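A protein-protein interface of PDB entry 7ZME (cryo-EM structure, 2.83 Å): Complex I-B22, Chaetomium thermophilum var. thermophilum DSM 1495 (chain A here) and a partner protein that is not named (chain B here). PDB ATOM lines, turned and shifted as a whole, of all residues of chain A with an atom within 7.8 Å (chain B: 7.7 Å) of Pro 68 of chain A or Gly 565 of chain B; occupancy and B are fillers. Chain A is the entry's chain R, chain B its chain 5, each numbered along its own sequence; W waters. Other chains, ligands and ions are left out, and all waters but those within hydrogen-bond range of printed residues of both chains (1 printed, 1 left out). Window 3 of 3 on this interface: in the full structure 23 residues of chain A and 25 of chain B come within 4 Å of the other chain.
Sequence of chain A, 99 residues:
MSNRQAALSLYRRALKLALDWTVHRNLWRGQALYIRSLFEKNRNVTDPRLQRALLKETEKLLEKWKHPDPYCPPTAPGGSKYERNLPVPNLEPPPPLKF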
ATOM      1  N   LEU A  17      22.977 -36.318  -1.595  1.00  0.00           N
ATOM      2  CA  LEU A  17      22.943 -35.631  -2.902  1.00  0.00           C
ATOM      3  C   LEU A  17      22.912 -36.663  -4.020  1.00  0.00           C
ATOM      4  O   LEU A  17      22.312 -36.368  -5.052  1.00  0.00           O
ATOM      5  CB  LEU A  17      24.222 -34.795  -2.980  1.00  0.00           C
ATOM      6  CG  LEU A  17      24.365 -33.900  -4.208  1.00  0.00           C
ATOM      7  CD1 LEU A  17      23.344 -32.775  -4.173  1.00  0.00           C
ATOM      8  CD2 LEU A  17      25.773 -33.334  -4.296  1.00  0.00           C
ATOM      9  N   ASP A  20      19.405 -37.678  -4.094  1.00  0.00           N
ATOM     10  CA  ASP A  20      18.552 -36.544  -4.550  1.00  0.00           C
ATOM     11  C   ASP A  20      18.581 -36.497  -6.069  1.00  0.00           C
ATOM     12  O   ASP A  20      17.533 -36.205  -6.641  1.00  0.00           O
ATOM     13  CB  ASP A  20      18.942 -35.199  -3.941  1.00  0.00           C
ATOM     14  CG  ASP A  20      18.552 -35.033  -2.488  1.00  0.00           C
ATOM     15  OD1 ASP A  20      17.606 -35.719  -2.055  1.00  0.00           O
ATOM     16  OD2 ASP A  20      19.209 -34.226  -1.800  1.00  0.00           O
ATOM     17  N   TRP A  21      19.733 -36.781  -6.677  1.00  0.00           N
ATOM     18  CA  TRP A  21      19.872 -36.761  -8.154  1.00  0.00           C
ATOM     19  C   TRP A  21      19.394 -38.068  -8.773  1.00  0.00           C
ATOM     20  O   TRP A  21      18.670 -37.995  -9.717  1.00  0.00           O
ATOM     21  CB  TRP A  21      21.323 -36.497  -8.538  1.00  0.00           C
ATOM     22  CG  TRP A  21      21.660 -35.060  -8.771  1.00  0.00           C
ATOM     23  CD1 TRP A  21      22.502 -34.280  -8.035  1.00  0.00           C
ATOM     24  CD2 TRP A  21      21.167 -34.230  -9.833  1.00  0.00           C
ATOM     25  NE1 TRP A  21      22.559 -33.020  -8.564  1.00  0.00           N
ATOM     26  CE2 TRP A  21      21.749 -32.958  -9.664  1.00  0.00           C
ATOM     27  CE3 TRP A  21      20.276 -34.426 -10.892  1.00  0.00           C
ATOM     28  CZ2 TRP A  21      21.467 -31.895 -10.517  1.00  0.00           C
ATOM     29  CZ3 TRP A  21      20.013 -33.378 -11.741  1.00  0.00           C
ATOM     30  CH2 TRP A  21      20.606 -32.131 -11.560  1.00  0.00           C
ATOM     31  N   TRP A  65      27.841 -30.113  -7.942  1.00  0.00           N
ATOM     32  CA  TRP A  65      26.773 -31.002  -8.376  1.00  0.00           C
ATOM     33  C   TRP A  65      25.571 -30.917  -7.444  1.00  0.00           C
ATOM     34  O   TRP A  65      24.877 -31.909  -7.221  1.00  0.00           O
ATOM     35  CB  TRP A  65      27.283 -32.438  -8.480  1.00  0.00           C
ATOM     36  CG  TRP A  65      28.508 -32.561  -9.322  1.00  0.00           C
ATOM     37  CD1 TRP A  65      29.798 -32.603  -8.890  1.00  0.00           C
ATOM     38  CD2 TRP A  65      28.558 -32.654 -10.746  1.00  0.00           C
ATOM     39  NE1 TRP A  65      30.650 -32.715  -9.957  1.00  0.00           N
ATOM     40  CE2 TRP A  65      29.913 -32.748 -11.111  1.00  0.00           C
ATOM     41  CE3 TRP A  65      27.586 -32.664 -11.752  1.00  0.00           C
ATOM     42  CZ2 TRP A  65      30.323 -32.855 -12.436  1.00  0.00           C
ATOM     43  CZ3 TRP A  65      27.993 -32.767 -13.065  1.00  0.00           C
ATOM     44  CH2 TRP A  65      29.349 -32.865 -13.397  1.00  0.00           C
ATOM     45  N   LYS A  66      25.314 -29.734  -6.895  1.00  0.00           N
ATOM     46  CA  LYS A  66      24.170 -29.549  -6.015  1.00  0.00           C
ATOM     47  C   LYS A  66      22.869 -29.705  -6.790  1.00  0.00           C
ATOM     48  O   LYS A  66      22.765 -29.304  -7.951  1.00  0.00           O
ATOM     49  CB  LYS A  66      24.224 -28.176  -5.349  1.00  0.00           C
ATOM     50  CG  LYS A  66      24.171 -27.010  -6.313  1.00  0.00           C
ATOM     51  CD  LYS A  66      23.953 -25.700  -5.578  1.00  0.00           C
ATOM     52  CE  LYS A  66      23.903 -24.533  -6.545  1.00  0.00           C
ATOM     53  NZ  LYS A  66      23.539 -23.267  -5.864  1.00  0.00           N
ATOM     54  N   HIS A  67      21.879 -30.303  -6.145  1.00  0.00           N
ATOM     55  CA  HIS A  67      20.596 -30.500  -6.791  1.00  0.00           C
ATOM     56  C   HIS A  67      19.822 -29.184  -6.839  1.00  0.00           C
ATOM     57  O   HIS A  67      19.918 -28.374  -5.911  1.00  0.00           O
ATOM     58  CB  HIS A  67      19.780 -31.561  -6.053  1.00  0.00           C
ATOM     59  CG  HIS A  67      18.777 -32.253  -6.917  1.00  0.00           C
ATOM     60  ND1 HIS A  67      17.453 -31.882  -6.962  1.00  0.00           N
ATOM     61  CD2 HIS A  67      18.911 -33.276  -7.791  1.00  0.00           C
ATOM     62  CE1 HIS A  67      16.810 -32.653  -7.819  1.00  0.00           C
ATOM     63  NE2 HIS A  67      17.672 -33.510  -8.335  1.00  0.00           N
ATOM     64  N   PRO A  68      19.059 -28.937  -7.907  1.00  0.00           N
ATOM     65  CA  PRO A  68      18.249 -27.710  -7.948  1.00  0.00           C
ATOM     66  C   PRO A  68      17.252 -27.619  -6.808  1.00  0.00           C
ATOM     67  O   PRO A  68      16.966 -26.518  -6.325  1.00  0.00           O
ATOM     68  CB  PRO A  68      17.561 -27.800  -9.312  1.00  0.00           C
ATOM     69  CG  PRO A  68      18.442 -28.678 -10.120  1.00  0.00           C
ATOM     70  CD  PRO A  68      18.995 -29.683  -9.173  1.00  0.00           C
ATOM     71  N   ASP A  69      16.710 -28.750  -6.361  1.00  0.00           N
ATOM     72  CA  ASP A  69      15.877 -28.797  -5.163  1.00  0.00           C
ATOM     73  C   ASP A  69      16.075 -30.142  -4.473  1.00  0.00           C
ATOM     74  O   ASP A  69      15.691 -31.193  -5.008  1.00  0.00           O
ATOM     75  CB  ASP A  69      14.409 -28.527  -5.486  1.00  0.00           C
ATOM     76  CG  ASP A  69      13.782 -29.598  -6.350  1.00  0.00           C
ATOM     77  OD1 ASP A  69      14.480 -30.147  -7.230  1.00  0.00           O
ATOM     78  OD2 ASP A  69      12.584 -29.890  -6.149  1.00  0.00           O
ATOM     79  N   PRO A  70      16.744 -30.197  -3.287  1.00  0.00           N
ATOM     80  CA  PRO A  70      16.875 -31.451  -2.542  1.00  0.00           C
ATOM     81  C   PRO A  70      15.602 -31.950  -1.850  1.00  0.00           C
ATOM     82  O   PRO A  70      14.735 -31.153  -1.594  1.00  0.00           O
ATOM     83  CB  PRO A  70      17.861 -31.098  -1.428  1.00  0.00           C
ATOM     84  CG  PRO A  70      18.598 -29.905  -1.947  1.00  0.00           C
ATOM     85  CD  PRO A  70      17.490 -29.122  -2.605  1.00  0.00           C
ATOM     86  N   PHE B 294      10.565 -31.583 -15.056  1.00  0.00           N
ATOM     87  CA  PHE B 294      11.679 -31.545 -14.121  1.00  0.00           C
ATOM     88  C   PHE B 294      11.257 -31.238 -12.694  1.00  0.00           C
ATOM     89  O   PHE B 294      12.122 -31.126 -11.820  1.00  0.00           O
ATOM     90  CB  PHE B 294      12.712 -30.514 -14.584  1.00  0.00           C
ATOM     91  CG  PHE B 294      13.349 -30.844 -15.900  1.00  0.00           C
ATOM     92  CD1 PHE B 294      12.665 -30.652 -17.087  1.00  0.00           C
ATOM     93  CD2 PHE B 294      14.636 -31.348 -15.950  1.00  0.00           C
ATOM     94  CE1 PHE B 294      13.253 -30.960 -18.294  1.00  0.00           C
ATOM     95  CE2 PHE B 294      15.226 -31.651 -17.156  1.00  0.00           C
ATOM     96  CZ  PHE B 294      14.534 -31.457 -18.328  1.00  0.00           C
ATOM     97  N   GLN B 296       9.907 -31.939  -8.985  1.00  0.00           N
ATOM     98  CA  GLN B 296       9.939 -33.063  -8.060  1.00  0.00           C
ATOM     99  C   GLN B 296       8.711 -33.131  -7.169  1.00  0.00           C
ATOM    100  O   GLN B 296       8.456 -34.180  -6.571  1.00  0.00           O
ATOM    101  CB  GLN B 296      11.195 -32.992  -7.188  1.00  0.00           C
ATOM    102  CG  GLN B 296      12.454 -32.694  -7.967  1.00  0.00           C
ATOM    103  CD  GLN B 296      12.765 -33.761  -8.984  1.00  0.00           C
ATOM    104  OE1 GLN B 296      12.659 -34.951  -8.701  1.00  0.00           O
ATOM    105  NE2 GLN B 296      13.137 -33.341 -10.185  1.00  0.00           N
ATOM    106  N   ARG B 357      10.144 -38.763  -5.214  1.00  0.00           N
ATOM    107  CA  ARG B 357      11.308 -39.575  -4.780  1.00  0.00           C
ATOM    108  C   ARG B 357      10.925 -40.517  -3.630  1.00  0.00           C
ATOM    109  O   ARG B 357      11.795 -41.273  -3.188  1.00  0.00           O
ATOM    110  CB  ARG B 357      12.480 -38.640  -4.473  1.00  0.00           C
ATOM    111  CG  ARG B 357      13.014 -37.908  -5.698  1.00  0.00           C
ATOM    112  CD  ARG B 357      14.044 -36.811  -5.483  1.00  0.00           C
ATOM    113  NE  ARG B 357      13.480 -35.539  -5.054  1.00  0.00           N
ATOM    114  CZ  ARG B 357      14.159 -34.402  -4.945  1.00  0.00           C
ATOM    115  NH1 ARG B 357      13.547 -33.305  -4.540  1.00  0.00           N
ATOM    116  NH2 ARG B 357      15.442 -34.358  -5.249  1.00  0.00           N
ATOM    117  N   PHE B 559      26.567 -30.727 -19.445  1.00  0.00           N
ATOM    118  CA  PHE B 559      25.537 -30.012 -20.190  1.00  0.00           C
ATOM    119  C   PHE B 559      24.148 -30.347 -19.666  1.00  0.00           C
ATOM    120  O   PHE B 559      23.327 -29.452 -19.432  1.00  0.00           O
ATOM    121  CB  PHE B 559      25.651 -30.348 -21.677  1.00  0.00           C
ATOM    122  CG  PHE B 559      24.415 -30.040 -22.468  1.00  0.00           C
ATOM    123  CD1 PHE B 559      23.995 -28.733 -22.642  1.00  0.00           C
ATOM    124  CD2 PHE B 559      23.674 -31.059 -23.040  1.00  0.00           C
ATOM    125  CE1 PHE B 559      22.858 -28.448 -23.373  1.00  0.00           C
ATOM    126  CE2 PHE B 559      22.536 -30.782 -23.769  1.00  0.00           C
ATOM    127  CZ  PHE B 559      22.127 -29.475 -23.937  1.00  0.00           C
ATOM    128  N   GLY B 560      23.866 -31.636 -19.469  1.00  0.00           N
ATOM    129  CA  GLY B 560      22.557 -32.030 -18.981  1.00  0.00           C
ATOM    130  C   GLY B 560      22.281 -31.568 -17.567  1.00  0.00           C
ATOM    131  O   GLY B 560      21.122 -31.393 -17.182  1.00  0.00           O
ATOM    132  N   TYR B 561      23.333 -31.372 -16.772  1.00  0.00           N
ATOM    133  CA  TYR B 561      23.155 -30.834 -15.428  1.00  0.00           C
ATOM    134  C   TYR B 561      22.564 -29.432 -15.471  1.00  0.00           C
ATOM    135  O   TYR B 561      21.664 -29.106 -14.688  1.00  0.00           O
ATOM    136  CB  TYR B 561      24.493 -30.830 -14.687  1.00  0.00           C
ATOM    137  CG  TYR B 561      24.472 -30.118 -13.350  1.00  0.00           C
ATOM    138  CD1 TYR B 561      24.717 -28.757 -13.259  1.00  0.00           C
ATOM    139  CD2 TYR B 561      24.216 -30.812 -12.178  1.00  0.00           C
ATOM    140  CE1 TYR B 561      24.699 -28.110 -12.048  1.00  0.00           C
ATOM    141  CE2 TYR B 561      24.201 -30.169 -10.961  1.00  0.00           C
ATOM    142  CZ  TYR B 561      24.441 -28.820 -10.903  1.00  0.00           C
ATOM    143  OH  TYR B 561      24.424 -28.173  -9.691  1.00  0.00           O
ATOM    144  N   ASN B 562      23.064 -28.586 -16.371  1.00  0.00           N
ATOM    145  CA  ASN B 562      22.616 -27.200 -16.392  1.00  0.00           C
ATOM    146  C   ASN B 562      21.190 -27.076 -16.907  1.00  0.00           C
ATOM    147  O   ASN B 562      20.411 -26.268 -16.392  1.00  0.00           O
ATOM    148  CB  ASN B 562      23.568 -26.347 -17.224  1.00  0.00           C
ATOM    149  CG  ASN B 562      24.952 -26.286 -16.632  1.00  0.00           C
ATOM    150  OD1 ASN B 562      25.914 -26.774 -17.217  1.00  0.00           O
ATOM    151  ND2 ASN B 562      25.061 -25.687 -15.453  1.00  0.00           N
ATOM    152  N   ILE B 563      20.821 -27.864 -17.919  1.00  0.00           N
ATOM    153  CA  ILE B 563      19.467 -27.741 -18.439  1.00  0.00           C
ATOM    154  C   ILE B 563      18.458 -28.440 -17.542  1.00  0.00           C
ATOM    155  O   ILE B 563      17.272 -28.091 -17.575  1.00  0.00           O
ATOM    156  CB  ILE B 563      19.348 -28.270 -19.878  1.00  0.00           C
ATOM    157  CG1 ILE B 563      19.375 -29.789 -19.918  1.00  0.00           C
ATOM    158  CG2 ILE B 563      20.472 -27.729 -20.740  1.00  0.00           C
ATOM    159  CD1 ILE B 563      18.984 -30.318 -21.262  1.00  0.00           C
ATOM    160  N   PHE B 564      18.888 -29.417 -16.743  1.00  0.00           N
ATOM    161  CA  PHE B 564      18.018 -29.930 -15.692  1.00  0.00           C
ATOM    162  C   PHE B 564      17.684 -28.830 -14.697  1.00  0.00           C
ATOM    163  O   PHE B 564      16.519 -28.636 -14.334  1.00  0.00           O
ATOM    164  CB  PHE B 564      18.677 -31.113 -14.985  1.00  0.00           C
ATOM    165  CG  PHE B 564      17.744 -31.885 -14.095  1.00  0.00           C
ATOM    166  CD1 PHE B 564      17.396 -31.406 -12.844  1.00  0.00           C
ATOM    167  CD2 PHE B 564      17.218 -33.091 -14.509  1.00  0.00           C
ATOM    168  CE1 PHE B 564      16.540 -32.114 -12.031  1.00  0.00           C
ATOM    169  CE2 PHE B 564      16.364 -33.800 -13.700  1.00  0.00           C
ATOM    170  CZ  PHE B 564      16.025 -33.311 -12.459  1.00  0.00           C
ATOM    171  N   GLY B 565      18.699 -28.089 -14.252  1.00  0.00           N
ATOM    172  CA  GLY B 565      18.470 -26.992 -13.335  1.00  0.00           C
ATOM    173  C   GLY B 565      17.874 -25.762 -13.970  1.00  0.00           C
ATOM    174  O   GLY B 565      17.274 -24.945 -13.265  1.00  0.00           O
ATOM    175  N   PHE B 566      18.027 -25.600 -15.284  1.00  0.00           N
ATOM    176  CA  PHE B 566      17.384 -24.475 -15.950  1.00  0.00           C
ATOM    177  C   PHE B 566      15.873 -24.643 -15.974  1.00  0.00           C
ATOM    178  O   PHE B 566      15.131 -23.675 -15.773  1.00  0.00           O
ATOM    179  CB  PHE B 566      17.928 -24.315 -17.368  1.00  0.00           C
ATOM    180  CG  PHE B 566      17.362 -23.136 -18.101  1.00  0.00           C
ATOM    181  CD1 PHE B 566      17.805 -21.858 -17.828  1.00  0.00           C
ATOM    182  CD2 PHE B 566      16.379 -23.305 -19.058  1.00  0.00           C
ATOM    183  CE1 PHE B 566      17.283 -20.776 -18.497  1.00  0.00           C
ATOM    184  CE2 PHE B 566      15.856 -22.225 -19.729  1.00  0.00           C
ATOM    185  CZ  PHE B 566      16.309 -20.960 -19.448  1.00  0.00           C
ATOM    186  N   PHE B 567      15.397 -25.862 -16.213  1.00  0.00           N
ATOM    187  CA  PHE B 567      13.966 -26.115 -16.302  1.00  0.00           C
ATOM    188  C   PHE B 567      13.342 -26.439 -14.956  1.00  0.00           C
ATOM    189  O   PHE B 567      12.166 -26.127 -14.739  1.00  0.00           O
ATOM    190  CB  PHE B 567      13.693 -27.252 -17.287  1.00  0.00           C
ATOM    191  CG  PHE B 567      14.017 -26.904 -18.706  1.00  0.00           C
ATOM    192  CD1 PHE B 567      13.530 -25.742 -19.272  1.00  0.00           C
ATOM    193  CD2 PHE B 567      14.809 -27.735 -19.475  1.00  0.00           C
ATOM    194  CE1 PHE B 567      13.826 -25.414 -20.572  1.00  0.00           C
ATOM    195  CE2 PHE B 567      15.108 -27.408 -20.780  1.00  0.00           C
ATOM    196  CZ  PHE B 567      14.616 -26.245 -21.328  1.00  0.00           C
ATOM    197  N   ASN B 568      14.097 -27.065 -14.050  1.00  0.00           N
ATOM    198  CA  ASN B 568      13.603 -27.252 -12.692  1.00  0.00           C
ATOM    199  C   ASN B 568      13.374 -25.909 -12.018  1.00  0.00           C
ATOM    200  O   ASN B 568      12.386 -25.724 -11.299  1.00  0.00           O
ATOM    201  CB  ASN B 568      14.588 -28.101 -11.890  1.00  0.00           C
ATOM    202  CG  ASN B 568      14.040 -28.522 -10.544  1.00  0.00           C
ATOM    203  OD1 ASN B 568      12.940 -28.143 -10.156  1.00  0.00           O
ATOM    204  ND2 ASN B 568      14.803 -29.332  -9.830  1.00  0.00           N
ATOM    205  N   GLN B 569      14.270 -24.954 -12.253  1.00  0.00           N
ATOM    206  CA  GLN B 569      14.149 -23.614 -11.707  1.00  0.00           C
ATOM    207  C   GLN B 569      13.289 -22.712 -12.573  1.00  0.00           C
ATOM    208  O   GLN B 569      13.408 -21.485 -12.484  1.00  0.00           O
ATOM    209  CB  GLN B 569      15.534 -23.003 -11.510  1.00  0.00           C
ATOM    210  CG  GLN B 569      16.325 -23.677 -10.415  1.00  0.00           C
ATOM    211  CD  GLN B 569      15.566 -23.713  -9.114  1.00  0.00           C
ATOM    212  OE1 GLN B 569      15.343 -22.680  -8.489  1.00  0.00           O
ATOM    213  NE2 GLN B 569      15.152 -24.904  -8.701  1.00  0.00           N
ATOM    214  N   ARG B 570      12.446 -23.298 -13.423  1.00  0.00           N
ATOM    215  CA  ARG B 570      11.330 -22.600 -14.052  1.00  0.00           C
ATOM    216  C   ARG B 570      11.818 -21.480 -14.966  1.00  0.00           C
ATOM    217  O   ARG B 570      11.337 -20.346 -14.905  1.00  0.00           O
ATOM    218  CB  ARG B 570      10.377 -22.060 -12.988  1.00  0.00           C
ATOM    219  CG  ARG B 570       9.924 -23.110 -12.003  1.00  0.00           C
ATOM    220  CD  ARG B 570       9.574 -22.474 -10.678  1.00  0.00           C
ATOM    221  NE  ARG B 570      10.718 -21.789 -10.082  1.00  0.00           N
ATOM    222  CZ  ARG B 570      11.591 -22.358  -9.257  1.00  0.00           C
ATOM    223  NH1 ARG B 570      11.460 -23.630  -8.917  1.00  0.00           N
ATOM    224  NH2 ARG B 570      12.596 -21.648  -8.769  1.00  0.00           N
ATOM    225  N   PHE B 571      12.797 -21.806 -15.809  1.00  0.00           N
ATOM    226  CA  PHE B 571      13.418 -20.867 -16.743  1.00  0.00           C
ATOM    227  C   PHE B 571      14.106 -19.711 -16.032  1.00  0.00           C
ATOM    228  O   PHE B 571      14.392 -18.685 -16.653  1.00  0.00           O
ATOM    229  CB  PHE B 571      12.404 -20.310 -17.750  1.00  0.00           C
ATOM    230  CG  PHE B 571      12.099 -21.230 -18.888  1.00  0.00           C
ATOM    231  CD1 PHE B 571      11.433 -22.421 -18.678  1.00  0.00           C
ATOM    232  CD2 PHE B 571      12.453 -20.887 -20.180  1.00  0.00           C
ATOM    233  CE1 PHE B 571      11.136 -23.258 -19.734  1.00  0.00           C
ATOM    234  CE2 PHE B 571      12.163 -21.722 -21.238  1.00  0.00           C
ATOM    235  CZ  PHE B 571      11.503 -22.908 -21.015  1.00  0.00           C
ATOM    236  N   LEU B 572      14.362 -19.855 -14.732  1.00  0.00           N
ATOM    237  CA  LEU B 572      15.008 -18.833 -13.908  1.00  0.00           C
ATOM    238  C   LEU B 572      14.198 -17.544 -13.837  1.00  0.00           C
ATOM    239  O   LEU B 572      14.720 -16.504 -13.432  1.00  0.00           O
ATOM    240  CB  LEU B 572      16.424 -18.537 -14.407  1.00  0.00           C
ATOM    241  CG  LEU B 572      17.289 -19.761 -14.698  1.00  0.00           C
ATOM    242  CD1 LEU B 572      18.634 -19.329 -15.212  1.00  0.00           C
ATOM    243  CD2 LEU B 572      17.441 -20.615 -13.456  1.00  0.00           C
HETATM  244  O   HOH W   1      15.890 -35.627  -9.383  1.00  0.00           O
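OD1 of Asp 69 of chain A lies within hydrogen-bond range of ND2 of Asn 568 of chain B, 2.7 Å away.
The backbone carbonyl oxygen of Lys 66 of chain A sits at hydrogen-bond distance from the side-chain hydroxyl of Tyr 561 of chain B (2.7 Å).
The side-chain carboxylate (OD2) of Asp 69 of chain A is in salt-bridge range of the guanidinium group (NH1) of Arg 357 of chain B (3.9 Å).
The guanidinium group (NH2) of Arg 357 of chain B sits at hydrogen-bond distance from the backbone carbonyl oxygen (O) of Asp 20 of chain A (3.1 Å).
The backbone carbonyl oxygen of Pro 68 of chain A sits at hydrogen-bond distance from the side-chain amide nitrogen of Gln 569 of chain B (3.4 Å).
The indole nitrogen (NE1) of Trp 21 of chain A is in hydrogen-bond range of the backbone carbonyl oxygen (O) of Trp 65 of chain A (2.9 Å).
OE1 of Gln 569 of chain B is in hydrogen-bond range of NH2 of Arg 570 of chain B.
The backbone carbonyl oxygen (O) of Asp 20 of chain A lies within hydrogen-bond range of a ring nitrogen (NE2) of His 67 of chain A (3.2 Å).
The backbone carbonyl oxygen of Asn 568 of chain B sits at hydrogen-bond distance from the guanidinium group of Arg 570 of chain B (3.3 Å).
The backbone carbonyl oxygen (O) of Phe 294 of chain B lies within hydrogen-bond range of the side-chain amide nitrogen (NE2) of Gln 296 of chain B, 2.9 Å away.
ND1 of His 67 of chain A is in hydrogen-bond range of O of Asp 69 of chain A, at 2.7 Å.
Trp 21 of chain A touches Tyr 561 of chain B.
CZ3 of Trp 21 of chain A touches CD1 of Phe 564 of chain B (3.5 Å).
C of Trp 65 of chain A touches OH of Tyr 561 of chain B (3.7 Å).
Arg 357 of chain B touches His 67 of chain A.
Phe 564 of chain B touches Pro 68 of chain A.
Pro 68 of chain A touches Gly 565 of chain B (CG to CA, 3.6 Å).
CB of Pro 68 of chain A touches ND2 of Asn 568 of chain B, 3.2 Å away.
OD1 of Asp 69 of chain A touches CG of Gln 296 of chain B (3.3 Å).
Pro 70 of chain A touches Arg 357 of chain B (C to NH1, 3.6 Å).
Of the printed residues of chain B, His 67 of chain A touches Arg 357 (3.4 Å).
Of the printed residues of chain B, Pro 68 of chain A touches Phe 564, Gly 565, Asn 568 and Gln 569.
Printed residues of chain B within 4 Å of Pro 70 of chain A: Arg 357 (3.6 Å).
Printed residues of chain A within 4 Å of Phe 564 of chain B: Trp 21 (3.5 Å) and Pro 68 (3.99 Å).
Of chain A, only Pro 68 (3.6 Å) comes within 4 Å of Gly 565 of chain B.
Printed residues of chain A within 4 Å of Asn 568 of chain B: Pro 68 and Asp 69.
Of the 9 printed residues of chain A, 8 touch a printed residue of chain B.
Hydrophobic or aromatic side chains of chain A that line the printed part of chain B: Trp 21, Trp 65, His 67 and Pro 68.
Along chain A the printed residues that touch a printed residue of chain B span positions 20 to 70.
Of the 17 printed residues of chain B, 7 touch a printed residue of chain A.
Printed residues of chain B that touch a printed residue of chain A: Gln 296, Arg 357, Tyr 561, Phe 564, Gly 565, Asn 568 and Gln 569.
Hydrophobic or aromatic side chains of chain B within 4 Å of the printed part of chain A: Tyr 561 and Phe 564.
Water W1 lies within hydrogen-bond range of NE2 of His 67 of chain A, O of Asp 20 of chain A and OE1 of Gln 296 of chain B.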
